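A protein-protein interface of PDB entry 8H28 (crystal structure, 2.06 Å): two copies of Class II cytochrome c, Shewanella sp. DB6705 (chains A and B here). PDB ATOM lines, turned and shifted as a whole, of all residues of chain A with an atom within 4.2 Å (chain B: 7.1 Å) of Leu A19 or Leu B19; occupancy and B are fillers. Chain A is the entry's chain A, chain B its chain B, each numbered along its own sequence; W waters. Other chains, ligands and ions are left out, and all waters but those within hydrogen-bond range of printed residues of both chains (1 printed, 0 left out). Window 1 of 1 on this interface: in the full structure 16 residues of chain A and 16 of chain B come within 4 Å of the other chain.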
ATOM      1  N   TYR A  12      10.125 -11.492 -22.744  1.00  0.00           N
ATOM      2  CA  TYR A  12       9.571 -12.375 -23.773  1.00  0.00           C
ATOM      3  C   TYR A  12       9.399 -13.797 -23.243  1.00  0.00           C
ATOM      4  O   TYR A  12       8.297 -14.354 -23.267  1.00  0.00           O
ATOM      5  CB  TYR A  12      10.470 -12.364 -25.013  1.00  0.00           C
ATOM      6  CG  TYR A  12       9.971 -13.212 -26.175  1.00  0.00           C
ATOM      7  CD1 TYR A  12       9.089 -12.687 -27.121  1.00  0.00           C
ATOM      8  CD2 TYR A  12      10.402 -14.522 -26.348  1.00  0.00           C
ATOM      9  CE1 TYR A  12       8.625 -13.463 -28.182  1.00  0.00           C
ATOM     10  CE2 TYR A  12       9.948 -15.304 -27.421  1.00  0.00           C
ATOM     11  CZ  TYR A  12       9.059 -14.765 -28.335  1.00  0.00           C
ATOM     12  OH  TYR A  12       8.606 -15.524 -29.404  1.00  0.00           O
ATOM     13  N   SER A  15       6.782 -14.028 -20.515  1.00  0.00           N
ATOM     14  CA  SER A  15       5.413 -13.962 -21.029  1.00  0.00           C
ATOM     15  C   SER A  15       4.972 -15.296 -21.619  1.00  0.00           C
ATOM     16  O   SER A  15       3.858 -15.755 -21.355  1.00  0.00           O
ATOM     17  CB  SER A  15       5.293 -12.860 -22.078  1.00  0.00           C
ATOM     18  OG  SER A  15       5.302 -11.605 -21.458  1.00  0.00           O
ATOM     19  N   ALA A  16       5.843 -15.929 -22.407  1.00  0.00           N
ATOM     20  CA  ALA A  16       5.532 -17.211 -23.023  1.00  0.00           C
ATOM     21  C   ALA A  16       5.240 -18.279 -21.967  1.00  0.00           C
ATOM     22  O   ALA A  16       4.259 -19.022 -22.076  1.00  0.00           O
ATOM     23  CB  ALA A  16       6.682 -17.625 -23.948  1.00  0.00           C
ATOM     24  N   PHE A  17       6.093 -18.387 -20.947  1.00  0.00           N
ATOM     25  CA  PHE A  17       5.814 -19.324 -19.863  1.00  0.00           C
ATOM     26  C   PHE A  17       4.506 -18.973 -19.170  1.00  0.00           C
ATOM     27  O   PHE A  17       3.728 -19.859 -18.788  1.00  0.00           O
ATOM     28  CB  PHE A  17       6.950 -19.325 -18.841  1.00  0.00           C
ATOM     29  CG  PHE A  17       8.226 -19.993 -19.321  1.00  0.00           C
ATOM     30  CD1 PHE A  17       8.224 -21.295 -19.800  1.00  0.00           C
ATOM     31  CD2 PHE A  17       9.442 -19.314 -19.246  1.00  0.00           C
ATOM     32  CE1 PHE A  17       9.417 -21.903 -20.220  1.00  0.00           C
ATOM     33  CE2 PHE A  17      10.631 -19.899 -19.669  1.00  0.00           C
ATOM     34  CZ  PHE A  17      10.616 -21.199 -20.159  1.00  0.00           C
ATOM     35  N   SER A  18       4.267 -17.687 -18.968  1.00  0.00           N
ATOM     36  CA  SER A  18       3.062 -17.252 -18.272  1.00  0.00           C
ATOM     37  C   SER A  18       1.799 -17.652 -19.032  1.00  0.00           C
ATOM     38  O   SER A  18       0.831 -18.127 -18.433  1.00  0.00           O
ATOM     39  CB  SER A  18       3.121 -15.740 -18.063  1.00  0.00           C
ATOM     40  OG  SER A  18       1.969 -15.277 -17.384  1.00  0.00           O
ATOM     41  N   LEU A  19       1.782 -17.448 -20.349  1.00  0.00           N
ATOM     42  CA  LEU A  19       0.623 -17.846 -21.142  1.00  0.00           C
ATOM     43  C   LEU A  19       0.506 -19.355 -21.182  1.00  0.00           C
ATOM     44  O   LEU A  19      -0.605 -19.899 -21.174  1.00  0.00           O
ATOM     45  CB  LEU A  19       0.715 -17.304 -22.564  1.00  0.00           C
ATOM     46  CG  LEU A  19       0.867 -15.798 -22.797  1.00  0.00           C
ATOM     47  CD1 LEU A  19       0.873 -15.491 -24.282  1.00  0.00           C
ATOM     48  CD2 LEU A  19      -0.207 -14.995 -22.098  1.00  0.00           C
ATOM     49  N   MET A  20       1.649 -20.049 -21.209  1.00  0.00           N
ATOM     50  CA  MET A  20       1.619 -21.507 -21.201  1.00  0.00           C
ATOM     51  C   MET A  20       0.978 -22.026 -19.925  1.00  0.00           C
ATOM     52  O   MET A  20       0.131 -22.931 -19.974  1.00  0.00           O
ATOM     53  CB  MET A  20       3.033 -22.063 -21.371  1.00  0.00           C
ATOM     54  CG  MET A  20       3.040 -23.484 -21.867  1.00  0.00           C
ATOM     55  SD  MET A  20       4.631 -24.031 -22.513  1.00  0.00           S
ATOM     56  CE  MET A  20       5.717 -23.349 -21.265  1.00  0.00           C
ATOM     57  N   ALA A  21       1.349 -21.442 -18.776  1.00  0.00           N
ATOM     58  CA  ALA A  21       0.798 -21.869 -17.494  1.00  0.00           C
ATOM     59  C   ALA A  21      -0.710 -21.707 -17.453  1.00  0.00           C
ATOM     60  O   ALA A  21      -1.431 -22.611 -16.999  1.00  0.00           O
ATOM     61  CB  ALA A  21       1.434 -21.080 -16.355  1.00  0.00           C
ATOM     62  N   HIS A  22      -1.211 -20.567 -17.933  1.00  0.00           N
ATOM     63  CA  HIS A  22      -2.653 -20.377 -17.957  1.00  0.00           C
ATOM     64  C   HIS A  22      -3.324 -21.473 -18.774  1.00  0.00           C
ATOM     65  O   HIS A  22      -4.309 -22.064 -18.340  1.00  0.00           O
ATOM     66  CB  HIS A  22      -3.010 -19.007 -18.516  1.00  0.00           C
ATOM     67  CG  HIS A  22      -4.477 -18.824 -18.746  1.00  0.00           C
ATOM     68  ND1 HIS A  22      -5.362 -18.595 -17.716  1.00  0.00           N
ATOM     69  CD2 HIS A  22      -5.219 -18.865 -19.881  1.00  0.00           C
ATOM     70  CE1 HIS A  22      -6.585 -18.477 -18.208  1.00  0.00           C
ATOM     71  NE2 HIS A  22      -6.525 -18.625 -19.521  1.00  0.00           N
ATOM     72  N   ASN A  23      -2.771 -21.802 -19.933  1.00  0.00           N
ATOM     73  CA  ASN A  23      -3.411 -22.824 -20.753  1.00  0.00           C
ATOM     74  C   ASN A  23      -3.226 -24.226 -20.180  1.00  0.00           C
ATOM     75  O   ASN A  23      -4.169 -25.035 -20.184  1.00  0.00           O
ATOM     76  CB  ASN A  23      -2.897 -22.710 -22.180  1.00  0.00           C
ATOM     77  CG  ASN A  23      -3.543 -21.540 -22.908  1.00  0.00           C
ATOM     78  OD1 ASN A  23      -4.664 -21.667 -23.399  1.00  0.00           O
ATOM     79  ND2 ASN A  23      -2.855 -20.381 -22.946  1.00  0.00           N
ATOM     80  N   LEU A  52       2.880 -22.530 -27.779  1.00  0.00           N
ATOM     81  CA  LEU A  52       3.623 -21.659 -26.873  1.00  0.00           C
ATOM     82  C   LEU A  52       4.955 -22.282 -26.450  1.00  0.00           C
ATOM     83  O   LEU A  52       5.929 -21.555 -26.233  1.00  0.00           O
ATOM     84  CB  LEU A  52       2.765 -21.319 -25.650  1.00  0.00           C
ATOM     85  CG  LEU A  52       1.592 -20.349 -25.819  1.00  0.00           C
ATOM     86  CD1 LEU A  52       0.587 -20.536 -24.683  1.00  0.00           C
ATOM     87  CD2 LEU A  52       2.050 -18.874 -25.903  1.00  0.00           C
ATOM     88  N   HIS B  11      -2.972  -8.932 -17.847  1.00  0.00           N
ATOM     89  CA  HIS B  11      -1.602  -9.390 -18.085  1.00  0.00           C
ATOM     90  C   HIS B  11      -1.558 -10.487 -19.148  1.00  0.00           C
ATOM     91  O   HIS B  11      -0.661 -10.503 -20.001  1.00  0.00           O
ATOM     92  CB  HIS B  11      -0.975  -9.887 -16.777  1.00  0.00           C
ATOM     93  CG  HIS B  11       0.415 -10.438 -16.940  1.00  0.00           C
ATOM     94  ND1 HIS B  11       0.670 -11.768 -17.203  1.00  0.00           N
ATOM     95  CD2 HIS B  11       1.628  -9.830 -16.880  1.00  0.00           C
ATOM     96  CE1 HIS B  11       1.975 -11.959 -17.291  1.00  0.00           C
ATOM     97  NE2 HIS B  11       2.580 -10.799 -17.097  1.00  0.00           N
ATOM     98  N   TYR B  12      -2.521 -11.413 -19.116  1.00  0.00           N
ATOM     99  CA  TYR B  12      -2.569 -12.462 -20.129  1.00  0.00           C
ATOM    100  C   TYR B  12      -2.704 -11.867 -21.534  1.00  0.00           C
ATOM    101  O   TYR B  12      -1.907 -12.173 -22.429  1.00  0.00           O
ATOM    102  CB  TYR B  12      -3.712 -13.436 -19.816  1.00  0.00           C
ATOM    103  CG  TYR B  12      -3.850 -14.587 -20.788  1.00  0.00           C
ATOM    104  CD1 TYR B  12      -3.125 -15.764 -20.616  1.00  0.00           C
ATOM    105  CD2 TYR B  12      -4.738 -14.509 -21.883  1.00  0.00           C
ATOM    106  CE1 TYR B  12      -3.263 -16.844 -21.523  1.00  0.00           C
ATOM    107  CE2 TYR B  12      -4.882 -15.580 -22.792  1.00  0.00           C
ATOM    108  CZ  TYR B  12      -4.137 -16.740 -22.605  1.00  0.00           C
ATOM    109  OH  TYR B  12      -4.259 -17.794 -23.482  1.00  0.00           O
ATOM    110  N   ARG B  13      -3.718 -11.021 -21.756  1.00  0.00           N
ATOM    111  CA  ARG B  13      -3.886 -10.458 -23.096  1.00  0.00           C
ATOM    112  C   ARG B  13      -2.705  -9.565 -23.471  1.00  0.00           C
ATOM    113  O   ARG B  13      -2.211  -9.624 -24.602  1.00  0.00           O
ATOM    114  CB  ARG B  13      -5.217  -9.697 -23.213  1.00  0.00           C
ATOM    115  CG  ARG B  13      -5.332  -8.395 -22.411  1.00  0.00           C
ATOM    116  CD  ARG B  13      -6.788  -8.042 -22.202  1.00  0.00           C
ATOM    117  NE  ARG B  13      -6.993  -6.713 -21.626  1.00  0.00           N
ATOM    118  CZ  ARG B  13      -8.037  -6.399 -20.865  1.00  0.00           C
ATOM    119  NH1 ARG B  13      -8.956  -7.321 -20.581  1.00  0.00           N
ATOM    120  NH2 ARG B  13      -8.162  -5.176 -20.377  1.00  0.00           N
ATOM    121  N   GLN B  14      -2.186  -8.785 -22.521  1.00  0.00           N
ATOM    122  CA  GLN B  14      -1.029  -7.940 -22.832  1.00  0.00           C
ATOM    123  C   GLN B  14       0.189  -8.774 -23.247  1.00  0.00           C
ATOM    124  O   GLN B  14       0.882  -8.440 -24.224  1.00  0.00           O
ATOM    125  CB  GLN B  14      -0.704  -7.056 -21.632  1.00  0.00           C
ATOM    126  CG  GLN B  14      -1.631  -5.851 -21.465  1.00  0.00           C
ATOM    127  CD  GLN B  14      -1.318  -5.045 -20.200  1.00  0.00           C
ATOM    128  OE1 GLN B  14      -0.664  -5.544 -19.280  1.00  0.00           O
ATOM    129  NE2 GLN B  14      -1.761  -3.793 -20.167  1.00  0.00           N
ATOM    130  N   SER B  15       0.455  -9.866 -22.522  1.00  0.00           N
ATOM    131  CA  SER B  15       1.564 -10.755 -22.857  1.00  0.00           C
ATOM    132  C   SER B  15       1.388 -11.353 -24.252  1.00  0.00           C
ATOM    133  O   SER B  15       2.345 -11.429 -25.030  1.00  0.00           O
ATOM    134  CB  SER B  15       1.665 -11.873 -21.815  1.00  0.00           C
ATOM    135  OG  SER B  15       2.114 -11.407 -20.552  1.00  0.00           O
ATOM    136  N   ALA B  16       0.182 -11.769 -24.571  1.00  0.00           N
ATOM    137  CA  ALA B  16      -0.108 -12.329 -25.867  1.00  0.00           C
ATOM    138  C   ALA B  16       0.200 -11.359 -26.995  1.00  0.00           C
ATOM    139  O   ALA B  16       0.877 -11.712 -27.915  1.00  0.00           O
ATOM    140  CB  ALA B  16      -1.530 -12.802 -25.926  1.00  0.00           C
ATOM    141  N   PHE B  17      -0.294 -10.137 -26.888  1.00  0.00           N
ATOM    142  CA  PHE B  17      -0.025  -9.101 -27.883  1.00  0.00           C
ATOM    143  C   PHE B  17       1.482  -8.818 -28.049  1.00  0.00           C
ATOM    144  O   PHE B  17       1.972  -8.723 -29.121  1.00  0.00           O
ATOM    145  CB  PHE B  17      -0.737  -7.822 -27.526  1.00  0.00           C
ATOM    146  CG  PHE B  17      -2.194  -7.844 -27.798  1.00  0.00           C
ATOM    147  CD1 PHE B  17      -2.661  -8.092 -29.049  1.00  0.00           C
ATOM    148  CD2 PHE B  17      -3.065  -7.602 -26.809  1.00  0.00           C
ATOM    149  CE1 PHE B  17      -3.988  -8.111 -29.307  1.00  0.00           C
ATOM    150  CE2 PHE B  17      -4.404  -7.608 -27.045  1.00  0.00           C
ATOM    151  CZ  PHE B  17      -4.868  -7.859 -28.303  1.00  0.00           C
ATOM    152  N   SER B  18       2.171  -8.680 -26.934  1.00  0.00           N
ATOM    153  CA  SER B  18       3.587  -8.431 -26.901  1.00  0.00           C
ATOM    154  C   SER B  18       4.354  -9.493 -27.650  1.00  0.00           C
ATOM    155  O   SER B  18       5.162  -9.175 -28.473  1.00  0.00           O
ATOM    156  CB  SER B  18       4.068  -8.348 -25.454  1.00  0.00           C
ATOM    157  OG  SER B  18       5.420  -8.061 -25.398  1.00  0.00           O
ATOM    158  N   LEU B  19       4.059 -10.756 -27.359  1.00  0.00           N
ATOM    159  CA  LEU B  19       4.723 -11.865 -28.036  1.00  0.00           C
ATOM    160  C   LEU B  19       4.346 -11.908 -29.511  1.00  0.00           C
ATOM    161  O   LEU B  19       5.182 -12.237 -30.359  1.00  0.00           O
ATOM    162  CB  LEU B  19       4.373 -13.198 -27.358  1.00  0.00           C
ATOM    163  CG  LEU B  19       4.660 -13.495 -25.884  1.00  0.00           C
ATOM    164  CD1 LEU B  19       4.145 -14.872 -25.502  1.00  0.00           C
ATOM    165  CD2 LEU B  19       6.133 -13.418 -25.591  1.00  0.00           C
ATOM    166  N   MET B  20       3.090 -11.598 -29.843  1.00  0.00           N
ATOM    167  CA  MET B  20       2.729 -11.529 -31.257  1.00  0.00           C
ATOM    168  C   MET B  20       3.525 -10.431 -31.949  1.00  0.00           C
ATOM    169  O   MET B  20       4.097 -10.643 -33.028  1.00  0.00           O
ATOM    170  CB  MET B  20       1.227 -11.280 -31.400  1.00  0.00           C
ATOM    171  CG  MET B  20       0.628 -11.628 -32.741  1.00  0.00           C
ATOM    172  SD  MET B  20      -1.195 -11.615 -32.694  1.00  0.00           S
ATOM    173  CE  MET B  20      -1.522 -10.131 -31.754  1.00  0.00           C
ATOM    174  N   ALA B  21       3.617  -9.259 -31.304  1.00  0.00           N
ATOM    175  CA  ALA B  21       4.366  -8.145 -31.871  1.00  0.00           C
ATOM    176  C   ALA B  21       5.824  -8.512 -32.105  1.00  0.00           C
ATOM    177  O   ALA B  21       6.426  -8.074 -33.093  1.00  0.00           O
ATOM    178  CB  ALA B  21       4.270  -6.922 -30.957  1.00  0.00           C
ATOM    179  N   HIS B  22       6.441  -9.247 -31.170  1.00  0.00           N
ATOM    180  CA  HIS B  22       7.839  -9.598 -31.391  1.00  0.00           C
ATOM    181  C   HIS B  22       7.986 -10.432 -32.655  1.00  0.00           C
ATOM    182  O   HIS B  22       8.891 -10.200 -33.467  1.00  0.00           O
ATOM    183  CB  HIS B  22       8.427 -10.332 -30.184  1.00  0.00           C
ATOM    184  CG  HIS B  22       9.803 -10.869 -30.430  1.00  0.00           C
ATOM    185  ND1 HIS B  22      10.919 -10.061 -30.464  1.00  0.00           N
ATOM    186  CD2 HIS B  22      10.244 -12.129 -30.659  1.00  0.00           C
ATOM    187  CE1 HIS B  22      11.988 -10.798 -30.709  1.00  0.00           C
ATOM    188  NE2 HIS B  22      11.606 -12.058 -30.823  1.00  0.00           N
ATOM    189  N   ASN B  23       7.104 -11.402 -32.839  1.00  0.00           N
ATOM    190  CA  ASN B  23       7.193 -12.267 -34.006  1.00  0.00           C
ATOM    191  C   ASN B  23       6.753 -11.539 -35.274  1.00  0.00           C
ATOM    192  O   ASN B  23       7.402 -11.649 -36.319  1.00  0.00           O
ATOM    193  CB  ASN B  23       6.372 -13.533 -33.743  1.00  0.00           C
ATOM    194  CG  ASN B  23       7.090 -14.485 -32.793  1.00  0.00           C
ATOM    195  OD1 ASN B  23       7.959 -15.248 -33.211  1.00  0.00           O
ATOM    196  ND2 ASN B  23       6.760 -14.411 -31.507  1.00  0.00           N
ATOM    197  N   PHE B  24       5.675 -10.764 -35.198  1.00  0.00           N
ATOM    198  CA  PHE B  24       5.246  -9.995 -36.362  1.00  0.00           C
ATOM    199  C   PHE B  24       6.324  -9.016 -36.825  1.00  0.00           C
ATOM    200  O   PHE B  24       6.601  -8.908 -38.026  1.00  0.00           O
ATOM    201  CB  PHE B  24       3.973  -9.224 -36.039  1.00  0.00           C
ATOM    202  CG  PHE B  24       3.339  -8.593 -37.244  1.00  0.00           C
ATOM    203  CD1 PHE B  24       2.845  -9.385 -38.276  1.00  0.00           C
ATOM    204  CD2 PHE B  24       3.279  -7.212 -37.368  1.00  0.00           C
ATOM    205  CE1 PHE B  24       2.265  -8.805 -39.385  1.00  0.00           C
ATOM    206  CE2 PHE B  24       2.700  -6.624 -38.474  1.00  0.00           C
ATOM    207  CZ  PHE B  24       2.189  -7.416 -39.487  1.00  0.00           C
ATOM    208  N   GLY B  25       6.939  -8.286 -35.879  1.00  0.00           N
ATOM    209  CA  GLY B  25       7.928  -7.265 -36.236  1.00  0.00           C
ATOM    210  C   GLY B  25       9.157  -7.823 -36.930  1.00  0.00           C
ATOM    211  O   GLY B  25       9.751  -7.157 -37.787  1.00  0.00           O
ATOM    212  N   ARG B  45       8.103 -17.572 -37.760  1.00  0.00           N
ATOM    213  CA  ARG B  45       7.450 -16.372 -37.249  1.00  0.00           C
ATOM    214  C   ARG B  45       5.971 -16.343 -37.615  1.00  0.00           C
ATOM    215  O   ARG B  45       5.130 -15.995 -36.780  1.00  0.00           O
ATOM    216  CB  ARG B  45       8.161 -15.123 -37.769  1.00  0.00           C
ATOM    217  CG  ARG B  45       9.635 -15.005 -37.377  1.00  0.00           C
ATOM    218  CD  ARG B  45       9.799 -14.976 -35.853  1.00  0.00           C
ATOM    219  NE  ARG B  45      11.156 -14.587 -35.441  1.00  0.00           N
ATOM    220  CZ  ARG B  45      11.586 -14.556 -34.187  1.00  0.00           C
ATOM    221  NH1 ARG B  45      10.782 -14.907 -33.181  1.00  0.00           N
ATOM    222  NH2 ARG B  45      12.837 -14.187 -33.941  1.00  0.00           N
ATOM    223  N   ASN B  48       4.077 -18.699 -35.426  1.00  0.00           N
ATOM    224  CA  ASN B  48       3.902 -18.135 -34.091  1.00  0.00           C
ATOM    225  C   ASN B  48       2.798 -17.073 -34.083  1.00  0.00           C
ATOM    226  O   ASN B  48       1.988 -17.010 -33.147  1.00  0.00           O
ATOM    227  CB  ASN B  48       5.226 -17.542 -33.608  1.00  0.00           C
ATOM    228  CG  ASN B  48       6.291 -18.596 -33.388  1.00  0.00           C
ATOM    229  OD1 ASN B  48       5.985 -19.775 -33.185  1.00  0.00           O
ATOM    230  ND2 ASN B  48       7.555 -18.180 -33.439  1.00  0.00           N
ATOM    231  N   VAL B  49       2.734 -16.239 -35.123  1.00  0.00           N
ATOM    232  CA  VAL B  49       1.719 -15.188 -35.150  1.00  0.00           C
ATOM    233  C   VAL B  49       0.322 -15.788 -35.280  1.00  0.00           C
ATOM    234  O   VAL B  49      -0.601 -15.403 -34.554  1.00  0.00           O
ATOM    235  CB  VAL B  49       2.023 -14.177 -36.264  1.00  0.00           C
ATOM    236  CG1 VAL B  49       0.842 -13.214 -36.442  1.00  0.00           C
ATOM    237  CG2 VAL B  49       3.306 -13.394 -35.920  1.00  0.00           C
ATOM    238  N   LEU B  52      -0.528 -17.240 -31.827  1.00  0.00           N
ATOM    239  CA  LEU B  52      -0.677 -16.225 -30.792  1.00  0.00           C
ATOM    240  C   LEU B  52      -1.902 -15.345 -31.025  1.00  0.00           C
ATOM    241  O   LEU B  52      -2.454 -14.797 -30.072  1.00  0.00           O
ATOM    242  CB  LEU B  52       0.588 -15.369 -30.726  1.00  0.00           C
ATOM    243  CG  LEU B  52       1.840 -16.039 -30.135  1.00  0.00           C
ATOM    244  CD1 LEU B  52       3.052 -15.267 -30.601  1.00  0.00           C
ATOM    245  CD2 LEU B  52       1.799 -16.123 -28.611  1.00  0.00           C
ATOM    246  N   LEU B  55      -5.050 -16.189 -28.842  1.00  0.00           N
ATOM    247  CA  LEU B  55      -4.958 -16.154 -27.384  1.00  0.00           C
ATOM    248  C   LEU B  55      -5.615 -14.932 -26.743  1.00  0.00           C
ATOM    249  O   LEU B  55      -6.333 -15.090 -25.742  1.00  0.00           O
ATOM    250  CB  LEU B  55      -3.480 -16.218 -26.958  1.00  0.00           C
ATOM    251  CG  LEU B  55      -2.742 -17.438 -27.531  1.00  0.00           C
ATOM    252  CD1 LEU B  55      -1.317 -17.564 -26.977  1.00  0.00           C
ATOM    253  CD2 LEU B  55      -3.519 -18.735 -27.284  1.00  0.00           C
HETATM  254  O   HOH W   1      -0.418 -14.221 -18.227  1.00  0.00           O
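Among the printed residues, pairs that only touch across the chains: Tyr A12 with His B22 (3.2 Å), His A22 with Tyr B12 (3.3 Å), Tyr A12 with Leu B19 (3.3 Å), Leu A19 with Tyr B12 (3.3 Å), Ser A18 with His B11 (3.3 Å), Leu A19 with Leu B19 (3.5 Å), Leu A19 with Ser B15 (3.7 Å), Ser A15 with Leu B19 (3.7 Å), Leu A19 with Ala B16 (3.7 Å), Ala A16 with Leu B19 (3.7 Å), Leu A52 with Leu B55 (3.8 Å) and Leu A52 with Leu B52 (3.9 Å).
Tyr A12 touches Leu B19, and with the chains exchanged Leu A19 touches Tyr B12.
Tyr A12 touches Asn B23, and with the chains exchanged Asn A23 touches Tyr B12.
Ser A15 touches its own counterpart, Ser B15.
Leu A19 touches its own counterpart, Leu B19.
Positions printed for both chains: 12, 15, 16, 17, 18, 19, 20, 21, 22, 23 and 52.
Of the 15 pairs that touch across the chains among the printed residues, 13 have their exchanged pair printed and touching as well.
O of Leu B19 lies within hydrogen-bond range of ND2 of Asn B23 (2.9 Å).
OD1 of Asn B23 sits at hydrogen-bond distance from ND2 of Asn B48 (3.0 Å).
The backbone carbonyl oxygen (O) of His B11 lies within hydrogen-bond range of the side-chain hydroxyl (OG) of Ser B15.
The backbone carbonyl oxygen (O) of Leu A19 is in hydrogen-bond range of the side-chain amide nitrogen (ND2) of Asn A23 (2.9 Å).
The side-chain amide oxygen (OD1) of Asn B23 is in hydrogen-bond range of the guanidinium group (NH1) of Arg B45 (2.8 Å).
OH of Tyr B12 lies within hydrogen-bond range of ND2 of Asn A23, 3.0 Å away.
OG of Ser B15 sits at hydrogen-bond distance from OG of Ser A15 (3.3 Å).
The side-chain amide nitrogen of Asn B23 is in hydrogen-bond range of the side-chain hydroxyl of Tyr A12, at 3.0 Å.
Water W1 bridges the side-chain hydroxyl of Ser A18 (2.7 Å) and a ring nitrogen (ND1) of His B11 (2.9 Å).
Printed residues of chain B within 4 Å of Asn A23: Tyr B12 (3.0 Å).
Gln B14 touches none of the printed residues of chain A.
Of the printed residues of chain A, Ala B16 touches Leu A19 (3.7 Å).
Leu B19 touches just these residues of chain A: Tyr A12, Ser A15, Ala A16 and Leu A19.
Of the printed residues of chain A, His B22 touches Tyr A12 (3.2 Å).
Of the printed residues of chain A, Leu B52 touches Leu A52.
Of the printed residues of chain A, Leu B55 touches Leu A52.
Printed residues of chain B that touch a printed residue of chain A: His B11, Tyr B12, Ser B15, Ala B16, Leu B19, His B22, Asn B23, Leu B52 and Leu B55.
Hydrophobic or aromatic side chains of chain B that line the printed part of chain A: His B11, Tyr B12, Ala B16, Leu B19, His B22, Leu B52 and Leu B55.
Among the printed residues, no Asp or Glu carboxylate lies within 4 Å of a Lys or Arg side-chain nitrogen of the other chain.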
